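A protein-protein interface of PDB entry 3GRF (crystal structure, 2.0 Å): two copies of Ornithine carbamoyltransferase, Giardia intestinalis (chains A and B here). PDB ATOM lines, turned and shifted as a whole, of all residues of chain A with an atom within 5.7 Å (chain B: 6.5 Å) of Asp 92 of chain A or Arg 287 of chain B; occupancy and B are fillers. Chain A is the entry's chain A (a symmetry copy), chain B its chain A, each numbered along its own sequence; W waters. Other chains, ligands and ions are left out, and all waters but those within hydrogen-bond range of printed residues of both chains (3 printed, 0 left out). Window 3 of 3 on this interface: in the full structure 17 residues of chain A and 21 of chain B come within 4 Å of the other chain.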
ATOM      1  N   THR A  89      -4.172  16.802 -21.707  1.00  0.00           N
ATOM      2  CA  THR A  89      -4.082  15.638 -20.809  1.00  0.00           C
ATOM      3  C   THR A  89      -2.747  15.733 -20.077  1.00  0.00           C
ATOM      4  O   THR A  89      -1.741  16.240 -20.629  1.00  0.00           O
ATOM      5  CB  THR A  89      -4.327  14.268 -21.593  1.00  0.00           C
ATOM      6  OG1 THR A  89      -5.633  13.763 -21.306  1.00  0.00           O
ATOM      7  CG2 THR A  89      -3.394  13.188 -21.236  1.00  0.00           C
ATOM      8  N   VAL A  90      -2.729  15.282 -18.831  1.00  0.00           N
ATOM      9  CA  VAL A  90      -1.473  15.250 -18.079  1.00  0.00           C
ATOM     10  C   VAL A  90      -0.523  14.154 -18.571  1.00  0.00           C
ATOM     11  O   VAL A  90       0.680  14.373 -18.623  1.00  0.00           O
ATOM     12  CB  VAL A  90      -1.650  15.286 -16.515  1.00  0.00           C
ATOM     13  CG1 VAL A  90      -3.053  14.910 -16.091  1.00  0.00           C
ATOM     14  CG2 VAL A  90      -0.605  14.446 -15.812  1.00  0.00           C
ATOM     15  N   GLN A  91      -1.074  13.000 -18.939  1.00  0.00           N
ATOM     16  CA  GLN A  91      -0.303  11.931 -19.588  1.00  0.00           C
ATOM     17  C   GLN A  91       0.429  12.410 -20.841  1.00  0.00           C
ATOM     18  O   GLN A  91       1.602  12.132 -21.005  1.00  0.00           O
ATOM     19  CB  GLN A  91      -1.218  10.742 -19.945  1.00  0.00           C
ATOM     20  CG  GLN A  91      -0.488   9.668 -20.748  1.00  0.00           C
ATOM     21  CD  GLN A  91      -1.407   8.585 -21.248  1.00  0.00           C
ATOM     22  OE1 GLN A  91      -0.962   7.622 -21.858  1.00  0.00           O
ATOM     23  NE2 GLN A  91      -2.706   8.721 -20.966  1.00  0.00           N
ATOM     24  N   ASP A  92      -0.320  13.076 -21.728  1.00  0.00           N
ATOM     25  CA  ASP A  92       0.156  13.614 -22.989  1.00  0.00           C
ATOM     26  C   ASP A  92       1.185  14.691 -22.727  1.00  0.00           C
ATOM     27  O   ASP A  92       2.241  14.716 -23.373  1.00  0.00           O
ATOM     28  CB  ASP A  92      -1.003  14.193 -23.806  1.00  0.00           C
ATOM     29  CG  ASP A  92      -1.887  13.116 -24.448  1.00  0.00           C
ATOM     30  OD1 ASP A  92      -1.646  11.893 -24.296  1.00  0.00           O
ATOM     31  OD2 ASP A  92      -2.836  13.501 -25.146  1.00  0.00           O
ATOM     32  N   THR A  93       0.908  15.557 -21.752  1.00  0.00           N
ATOM     33  CA  THR A  93       1.868  16.582 -21.378  1.00  0.00           C
ATOM     34  C   THR A  93       3.175  15.897 -20.930  1.00  0.00           C
ATOM     35  O   THR A  93       4.248  16.159 -21.493  1.00  0.00           O
ATOM     36  CB  THR A  93       1.274  17.535 -20.311  1.00  0.00           C
ATOM     37  OG1 THR A  93       0.124  18.188 -20.856  1.00  0.00           O
ATOM     38  CG2 THR A  93       2.269  18.584 -19.910  1.00  0.00           C
ATOM     39  N   ALA A  94       3.071  14.974 -19.964  1.00  0.00           N
ATOM     40  CA  ALA A  94       4.249  14.309 -19.421  1.00  0.00           C
ATOM     41  C   ALA A  94       4.984  13.477 -20.477  1.00  0.00           C
ATOM     42  O   ALA A  94       6.197  13.477 -20.526  1.00  0.00           O
ATOM     43  CB  ALA A  94       3.883  13.468 -18.204  1.00  0.00           C
ATOM     44  N   GLU A  95       4.233  12.752 -21.310  1.00  0.00           N
ATOM     45  CA  GLU A  95       4.799  11.963 -22.413  1.00  0.00           C
ATOM     46  C   GLU A  95       5.582  12.857 -23.345  1.00  0.00           C
ATOM     47  O   GLU A  95       6.636  12.493 -23.839  1.00  0.00           O
ATOM     48  CB  GLU A  95       3.708  11.212 -23.201  1.00  0.00           C
ATOM     49  CG  GLU A  95       3.149   9.943 -22.516  1.00  0.00           C
ATOM     50  CD  GLU A  95       4.070   8.716 -22.576  1.00  0.00           C
ATOM     51  OE1 GLU A  95       3.629   7.612 -22.173  1.00  0.00           O
ATOM     52  OE2 GLU A  95       5.219   8.812 -23.016  1.00  0.00           O
ATOM     53  N   VAL A  96       5.072  14.058 -23.540  1.00  0.00           N
ATOM     54  CA  VAL A  96       5.685  14.982 -24.477  1.00  0.00           C
ATOM     55  C   VAL A  96       6.897  15.699 -23.875  1.00  0.00           C
ATOM     56  O   VAL A  96       7.883  15.874 -24.568  1.00  0.00           O
ATOM     57  CB  VAL A  96       4.635  15.967 -24.996  1.00  0.00           C
ATOM     58  CG1 VAL A  96       5.280  17.174 -25.621  1.00  0.00           C
ATOM     59  CG2 VAL A  96       3.647  15.224 -25.960  1.00  0.00           C
ATOM     60  N   PHE A  97       6.832  16.137 -22.610  1.00  0.00           N
ATOM     61  CA  PHE A  97       8.013  16.831 -22.048  1.00  0.00           C
ATOM     62  C   PHE A  97       9.193  15.906 -21.767  1.00  0.00           C
ATOM     63  O   PHE A  97      10.325  16.347 -21.797  1.00  0.00           O
ATOM     64  CB  PHE A  97       7.728  17.871 -20.915  1.00  0.00           C
ATOM     65  CG  PHE A  97       7.151  17.311 -19.594  1.00  0.00           C
ATOM     66  CD1 PHE A  97       5.879  17.737 -19.152  1.00  0.00           C
ATOM     67  CD2 PHE A  97       7.884  16.455 -18.771  1.00  0.00           C
ATOM     68  CE1 PHE A  97       5.352  17.297 -17.919  1.00  0.00           C
ATOM     69  CE2 PHE A  97       7.374  15.996 -17.543  1.00  0.00           C
ATOM     70  CZ  PHE A  97       6.112  16.418 -17.115  1.00  0.00           C
ATOM     71  N   LEU B  56       2.582  24.709 -24.582  1.00  0.00           N
ATOM     72  CA  LEU B  56       3.587  23.957 -23.887  1.00  0.00           C
ATOM     73  C   LEU B  56       4.578  23.441 -24.896  1.00  0.00           C
ATOM     74  O   LEU B  56       5.765  23.636 -24.731  1.00  0.00           O
ATOM     75  CB  LEU B  56       2.943  22.781 -23.143  1.00  0.00           C
ATOM     76  CG  LEU B  56       3.952  21.970 -22.320  1.00  0.00           C
ATOM     77  CD1 LEU B  56       3.593  22.007 -20.854  1.00  0.00           C
ATOM     78  CD2 LEU B  56       4.016  20.569 -22.853  1.00  0.00           C
ATOM     79  N   ARG B  57       4.077  22.770 -25.936  1.00  0.00           N
ATOM     80  CA  ARG B  57       4.901  22.211 -27.014  1.00  0.00           C
ATOM     81  C   ARG B  57       5.838  23.237 -27.609  1.00  0.00           C
ATOM     82  O   ARG B  57       7.029  22.985 -27.756  1.00  0.00           O
ATOM     83  CB  ARG B  57       4.038  21.665 -28.154  1.00  0.00           C
ATOM     84  CG  ARG B  57       3.766  20.182 -28.096  1.00  0.00           C
ATOM     85  CD  ARG B  57       2.429  19.952 -28.795  1.00  0.00           C
ATOM     86  NE  ARG B  57       1.426  19.529 -27.843  1.00  0.00           N
ATOM     87  CZ  ARG B  57       0.793  20.321 -26.974  1.00  0.00           C
ATOM     88  NH1 ARG B  57       1.046  21.623 -26.899  1.00  0.00           N
ATOM     89  NH2 ARG B  57      -0.096  19.789 -26.149  1.00  0.00           N
ATOM     90  N   GLN B 264     -13.841  11.997 -38.945  1.00  0.00           N
ATOM     91  CA  GLN B 264     -13.137  11.477 -37.772  1.00  0.00           C
ATOM     92  C   GLN B 264     -12.220  10.372 -38.229  1.00  0.00           C
ATOM     93  O   GLN B 264     -12.660   9.479 -38.960  1.00  0.00           O
ATOM     94  CB  GLN B 264     -14.156  10.882 -36.811  1.00  0.00           C
ATOM     95  CG  GLN B 264     -13.528  10.203 -35.601  1.00  0.00           C
ATOM     96  CD  GLN B 264     -14.544   9.928 -34.561  1.00  0.00           C
ATOM     97  OE1 GLN B 264     -15.313   8.998 -34.684  1.00  0.00           O
ATOM     98  NE2 GLN B 264     -14.599  10.771 -33.554  1.00  0.00           N
ATOM     99  N   LEU B 283      -1.207  17.751 -32.141  1.00  0.00           N
ATOM    100  CA  LEU B 283      -1.660  17.993 -30.744  1.00  0.00           C
ATOM    101  C   LEU B 283      -2.079  19.455 -30.486  1.00  0.00           C
ATOM    102  O   LEU B 283      -1.709  20.336 -31.239  1.00  0.00           O
ATOM    103  CB  LEU B 283      -0.645  17.508 -29.687  1.00  0.00           C
ATOM    104  CG  LEU B 283      -0.206  16.030 -29.730  1.00  0.00           C
ATOM    105  CD1 LEU B 283       0.901  15.703 -28.707  1.00  0.00           C
ATOM    106  CD2 LEU B 283      -1.415  15.083 -29.589  1.00  0.00           C
ATOM    107  N   PRO B 284      -2.890  19.712 -29.441  1.00  0.00           N
ATOM    108  CA  PRO B 284      -3.558  18.806 -28.492  1.00  0.00           C
ATOM    109  C   PRO B 284      -4.554  17.840 -29.151  1.00  0.00           C
ATOM    110  O   PRO B 284      -5.315  18.237 -30.055  1.00  0.00           O
ATOM    111  CB  PRO B 284      -4.292  19.772 -27.556  1.00  0.00           C
ATOM    112  CG  PRO B 284      -4.480  20.992 -28.372  1.00  0.00           C
ATOM    113  CD  PRO B 284      -3.216  21.117 -29.143  1.00  0.00           C
ATOM    114  N   ALA B 285      -4.508  16.579 -28.723  1.00  0.00           N
ATOM    115  CA  ALA B 285      -5.429  15.536 -29.181  1.00  0.00           C
ATOM    116  C   ALA B 285      -6.692  15.471 -28.317  1.00  0.00           C
ATOM    117  O   ALA B 285      -6.607  15.443 -27.085  1.00  0.00           O
ATOM    118  CB  ALA B 285      -4.735  14.177 -29.162  1.00  0.00           C
ATOM    119  N   THR B 286      -7.857  15.431 -28.966  1.00  0.00           N
ATOM    120  CA  THR B 286      -9.118  15.111 -28.291  1.00  0.00           C
ATOM    121  C   THR B 286      -9.672  13.770 -28.787  1.00  0.00           C
ATOM    122  O   THR B 286     -10.222  13.663 -29.898  1.00  0.00           O
ATOM    123  CB  THR B 286     -10.156  16.240 -28.466  1.00  0.00           C
ATOM    124  OG1 THR B 286      -9.550  17.477 -28.100  1.00  0.00           O
ATOM    125  CG2 THR B 286     -11.374  16.015 -27.591  1.00  0.00           C
ATOM    126  N   ARG B 287      -9.542  12.768 -27.926  1.00  0.00           N
ATOM    127  CA  ARG B 287      -9.730  11.353 -28.283  1.00  0.00           C
ATOM    128  C   ARG B 287     -11.029  10.933 -28.896  1.00  0.00           C
ATOM    129  O   ARG B 287     -11.074   9.847 -29.462  1.00  0.00           O
ATOM    130  CB  ARG B 287      -9.465  10.434 -27.104  1.00  0.00           C
ATOM    131  CG  ARG B 287      -7.998  10.133 -26.913  1.00  0.00           C
ATOM    132  CD  ARG B 287      -7.460  10.777 -25.653  1.00  0.00           C
ATOM    133  NE  ARG B 287      -6.010  11.040 -25.690  1.00  0.00           N
ATOM    134  CZ  ARG B 287      -5.103  10.107 -25.960  1.00  0.00           C
ATOM    135  NH1 ARG B 287      -5.499   8.867 -26.240  1.00  0.00           N
ATOM    136  NH2 ARG B 287      -3.819  10.409 -25.969  1.00  0.00           N
ATOM    137  N   GLY B 288     -12.095  11.708 -28.772  1.00  0.00           N
ATOM    138  CA  GLY B 288     -13.342  11.329 -29.468  1.00  0.00           C
ATOM    139  C   GLY B 288     -13.829  12.347 -30.475  1.00  0.00           C
ATOM    140  O   GLY B 288     -15.000  12.307 -30.883  1.00  0.00           O
ATOM    141  N   GLU B 289     -12.948  13.278 -30.856  1.00  0.00           N
ATOM    142  CA  GLU B 289     -13.269  14.260 -31.897  1.00  0.00           C
ATOM    143  C   GLU B 289     -12.560  13.924 -33.198  1.00  0.00           C
ATOM    144  O   GLU B 289     -13.049  13.100 -33.951  1.00  0.00           O
ATOM    145  CB  GLU B 289     -13.012  15.686 -31.396  1.00  0.00           C
ATOM    146  CG  GLU B 289     -13.840  15.960 -30.133  1.00  0.00           C
ATOM    147  CD  GLU B 289     -13.992  17.427 -29.784  1.00  0.00           C
ATOM    148  OE1 GLU B 289     -13.208  18.245 -30.325  1.00  0.00           O
ATOM    149  OE2 GLU B 289     -14.908  17.755 -28.972  1.00  0.00           O
ATOM    150  N   GLU B 290     -11.397  14.513 -33.448  1.00  0.00           N
ATOM    151  CA  GLU B 290     -10.726  14.340 -34.746  1.00  0.00           C
ATOM    152  C   GLU B 290     -10.258  12.896 -34.970  1.00  0.00           C
ATOM    153  O   GLU B 290     -10.104  12.448 -36.121  1.00  0.00           O
ATOM    154  CB  GLU B 290      -9.572  15.337 -34.899  1.00  0.00           C
ATOM    155  CG  GLU B 290      -8.409  15.126 -33.926  1.00  0.00           C
ATOM    156  CD  GLU B 290      -8.579  15.817 -32.583  1.00  0.00           C
ATOM    157  OE1 GLU B 290      -7.659  15.721 -31.751  1.00  0.00           O
ATOM    158  OE2 GLU B 290      -9.599  16.489 -32.344  1.00  0.00           O
ATOM    159  N   GLN B 291     -10.072  12.156 -33.875  1.00  0.00           N
ATOM    160  CA  GLN B 291      -9.815  10.708 -33.991  1.00  0.00           C
ATOM    161  C   GLN B 291     -10.302   9.911 -32.781  1.00  0.00           C
ATOM    162  O   GLN B 291     -10.576  10.494 -31.748  1.00  0.00           O
ATOM    163  CB  GLN B 291      -8.347  10.431 -34.267  1.00  0.00           C
ATOM    164  CG  GLN B 291      -7.429  11.538 -33.758  1.00  0.00           C
ATOM    165  CD  GLN B 291      -7.128  11.348 -32.346  1.00  0.00           C
ATOM    166  OE1 GLN B 291      -7.230  12.259 -31.514  1.00  0.00           O
ATOM    167  NE2 GLN B 291      -6.807  10.120 -32.025  1.00  0.00           N
ATOM    168  N   THR B 292     -10.451   8.596 -32.943  1.00  0.00           N
ATOM    169  CA  THR B 292     -10.780   7.710 -31.836  1.00  0.00           C
ATOM    170  C   THR B 292      -9.566   7.414 -31.002  1.00  0.00           C
ATOM    171  O   THR B 292      -8.449   7.539 -31.486  1.00  0.00           O
ATOM    172  CB  THR B 292     -11.427   6.386 -32.298  1.00  0.00           C
ATOM    173  OG1 THR B 292     -10.501   5.607 -33.067  1.00  0.00           O
ATOM    174  CG2 THR B 292     -12.690   6.638 -33.127  1.00  0.00           C
ATOM    175  N   ALA B 293      -9.804   7.039 -29.743  1.00  0.00           N
ATOM    176  CA  ALA B 293      -8.746   6.731 -28.817  1.00  0.00           C
ATOM    177  C   ALA B 293      -7.976   5.497 -29.325  1.00  0.00           C
ATOM    178  O   ALA B 293      -6.752   5.433 -29.214  1.00  0.00           O
ATOM    179  CB  ALA B 293      -9.317   6.528 -27.381  1.00  0.00           C
ATOM    180  N   SER B 294      -8.673   4.573 -29.979  1.00  0.00           N
ATOM    181  CA  SER B 294      -8.048   3.389 -30.582  1.00  0.00           C
ATOM    182  C   SER B 294      -7.019   3.696 -31.681  1.00  0.00           C
ATOM    183  O   SER B 294      -6.146   2.889 -31.934  1.00  0.00           O
ATOM    184  CB  SER B 294      -9.092   2.450 -31.167  1.00  0.00           C
ATOM    185  OG  SER B 294      -9.597   2.968 -32.378  1.00  0.00           O
ATOM    186  N   ILE B 296      -5.265   6.918 -31.950  1.00  0.00           N
ATOM    187  CA  ILE B 296      -4.154   7.639 -31.314  1.00  0.00           C
ATOM    188  C   ILE B 296      -3.358   6.819 -30.323  1.00  0.00           C
ATOM    189  O   ILE B 296      -2.159   7.047 -30.156  1.00  0.00           O
ATOM    190  CB  ILE B 296      -4.578   9.015 -30.700  1.00  0.00           C
ATOM    191  CG1 ILE B 296      -3.360   9.771 -30.112  1.00  0.00           C
ATOM    192  CG2 ILE B 296      -5.750   8.859 -29.697  1.00  0.00           C
ATOM    193  CD1 ILE B 296      -3.460  11.303 -30.162  1.00  0.00           C
ATOM    194  N   ASP B 297      -4.020   5.866 -29.676  1.00  0.00           N
ATOM    195  CA  ASP B 297      -3.359   5.010 -28.687  1.00  0.00           C
ATOM    196  C   ASP B 297      -3.062   3.652 -29.302  1.00  0.00           C
ATOM    197  O   ASP B 297      -2.497   2.766 -28.654  1.00  0.00           O
ATOM    198  CB  ASP B 297      -4.223   4.864 -27.431  1.00  0.00           C
ATOM    199  CG  ASP B 297      -4.525   6.196 -26.770  1.00  0.00           C
ATOM    200  OD1 ASP B 297      -3.670   7.118 -26.752  1.00  0.00           O
ATOM    201  OD2 ASP B 297      -5.640   6.336 -26.260  1.00  0.00           O
ATOM    202  N   TYR B 304       3.413  11.022 -30.041  1.00  0.00           N
ATOM    203  CA  TYR B 304       4.260  11.518 -28.961  1.00  0.00           C
ATOM    204  C   TYR B 304       5.718  11.706 -29.434  1.00  0.00           C
ATOM    205  O   TYR B 304       6.389  12.617 -28.985  1.00  0.00           O
ATOM    206  CB  TYR B 304       4.300  10.535 -27.797  1.00  0.00           C
ATOM    207  CG  TYR B 304       3.082  10.364 -26.924  1.00  0.00           C
ATOM    208  CD1 TYR B 304       2.851   9.143 -26.311  1.00  0.00           C
ATOM    209  CD2 TYR B 304       2.180  11.391 -26.699  1.00  0.00           C
ATOM    210  CE1 TYR B 304       1.786   8.935 -25.482  1.00  0.00           C
ATOM    211  CE2 TYR B 304       1.075  11.192 -25.868  1.00  0.00           C
ATOM    212  CZ  TYR B 304       0.888   9.952 -25.268  1.00  0.00           C
ATOM    213  OH  TYR B 304      -0.163   9.705 -24.430  1.00  0.00           O
HETATM  214  O   HOH W   1       0.903  19.411 -23.397  1.00  0.00           O
HETATM  215  O   HOH W   2      -2.859  16.202 -26.577  1.00  0.00           O
HETATM  216  O   HOH W   3      -3.994   6.711 -23.195  1.00  0.00           O
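OH of Tyr 304 of chain B lies within hydrogen-bond range of OD1 of Asp 92 of chain A (2.6 Å).
The side-chain carboxylate of Asp 92 of chain A is in salt-bridge range of the guanidinium group of Arg 287 of chain B, at 3.1 Å.
OE1 of Gln 91 of chain A is in hydrogen-bond range of OH of Tyr 304 of chain B (3.4 Å).
The backbone carbonyl oxygen (O) of Arg 287 of chain B sits at hydrogen-bond distance from the backbone NH (N) of Ala 293 of chain B (3.1 Å).
The side-chain carboxylate (OD2) of Asp 297 of chain B is in salt-bridge range of the guanidinium group (NH1) of Arg 287 of chain B, at 2.5 Å.
The backbone carbonyl oxygen (O) of Thr 89 of chain A lies within hydrogen-bond range of the side-chain hydroxyl (OG1) of Thr 93 of chain A (2.7 Å).
Among the printed residues, pairs that only touch across the chains: Thr 93 of chain A with Leu 56 of chain B (3.8 Å), Glu 95 of chain A with Tyr 304 of chain B (3.4 Å) and Val 96 of chain A with Leu 283 of chain B (3.9 Å).
Of chain B, only Arg 287 (3.1 Å) and Tyr 304 (2.6 Å) come within 4 Å of Asp 92 of chain A.
Arg 287 of chain B touches one residue of chain A.
Printed residues of chain B within 4 Å of Glu 95 of chain A: Tyr 304 (3.4 Å).
Of the printed residues of chain A, Tyr 304 of chain B touches Gln 91 (3.4 Å), Asp 92 (2.6 Å) and Glu 95 (3.4 Å).
Of the printed residues of chain B, Thr 93 of chain A touches Leu 56.
Pro 284 of chain B touches none of the printed residues of chain A.
The nearest residue of chain B that does not touch Asp 92 of chain A is Ala 285 of chain B (4.5 Å).
Of the 18 printed residues of chain B, 4 touch a printed residue of chain A.
Of the 9 printed residues of chain A, 5 touch a printed residue of chain B.
Hydrophobic or aromatic side chains of chain A within 4 Å of the printed part of chain B: Val 96.
Among the printed residues, 6 pairs touch across the chains.
Among the printed residues, Asp or Glu carboxylates within 4 Å of a Lys or Arg side-chain nitrogen of the other chain: Asp 92 of chain A with Arg 287 of chain B (3.1 Å).
No position is printed for both chains.
Of the 6 pairs that touch across the chains among the printed residues, none has its exchanged pair printed and touching as well.
Water W2 lies within hydrogen-bond range of the backbone NH (N) of Ala 285 of chain B and the side-chain carboxylate (OD2) of Asp 92 of chain A.
Water W1 bridges OG1 of Thr 93 of chain A (2.9 Å) and NH2 of Arg 57 of chain B (3.0 Å).
Water W3 bridges the side-chain amide nitrogen (NE2) of Gln 91 of chain A (3.3 Å) and the side-chain carboxylate (OD2) of Asp 297 of chain B (3.5 Å).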
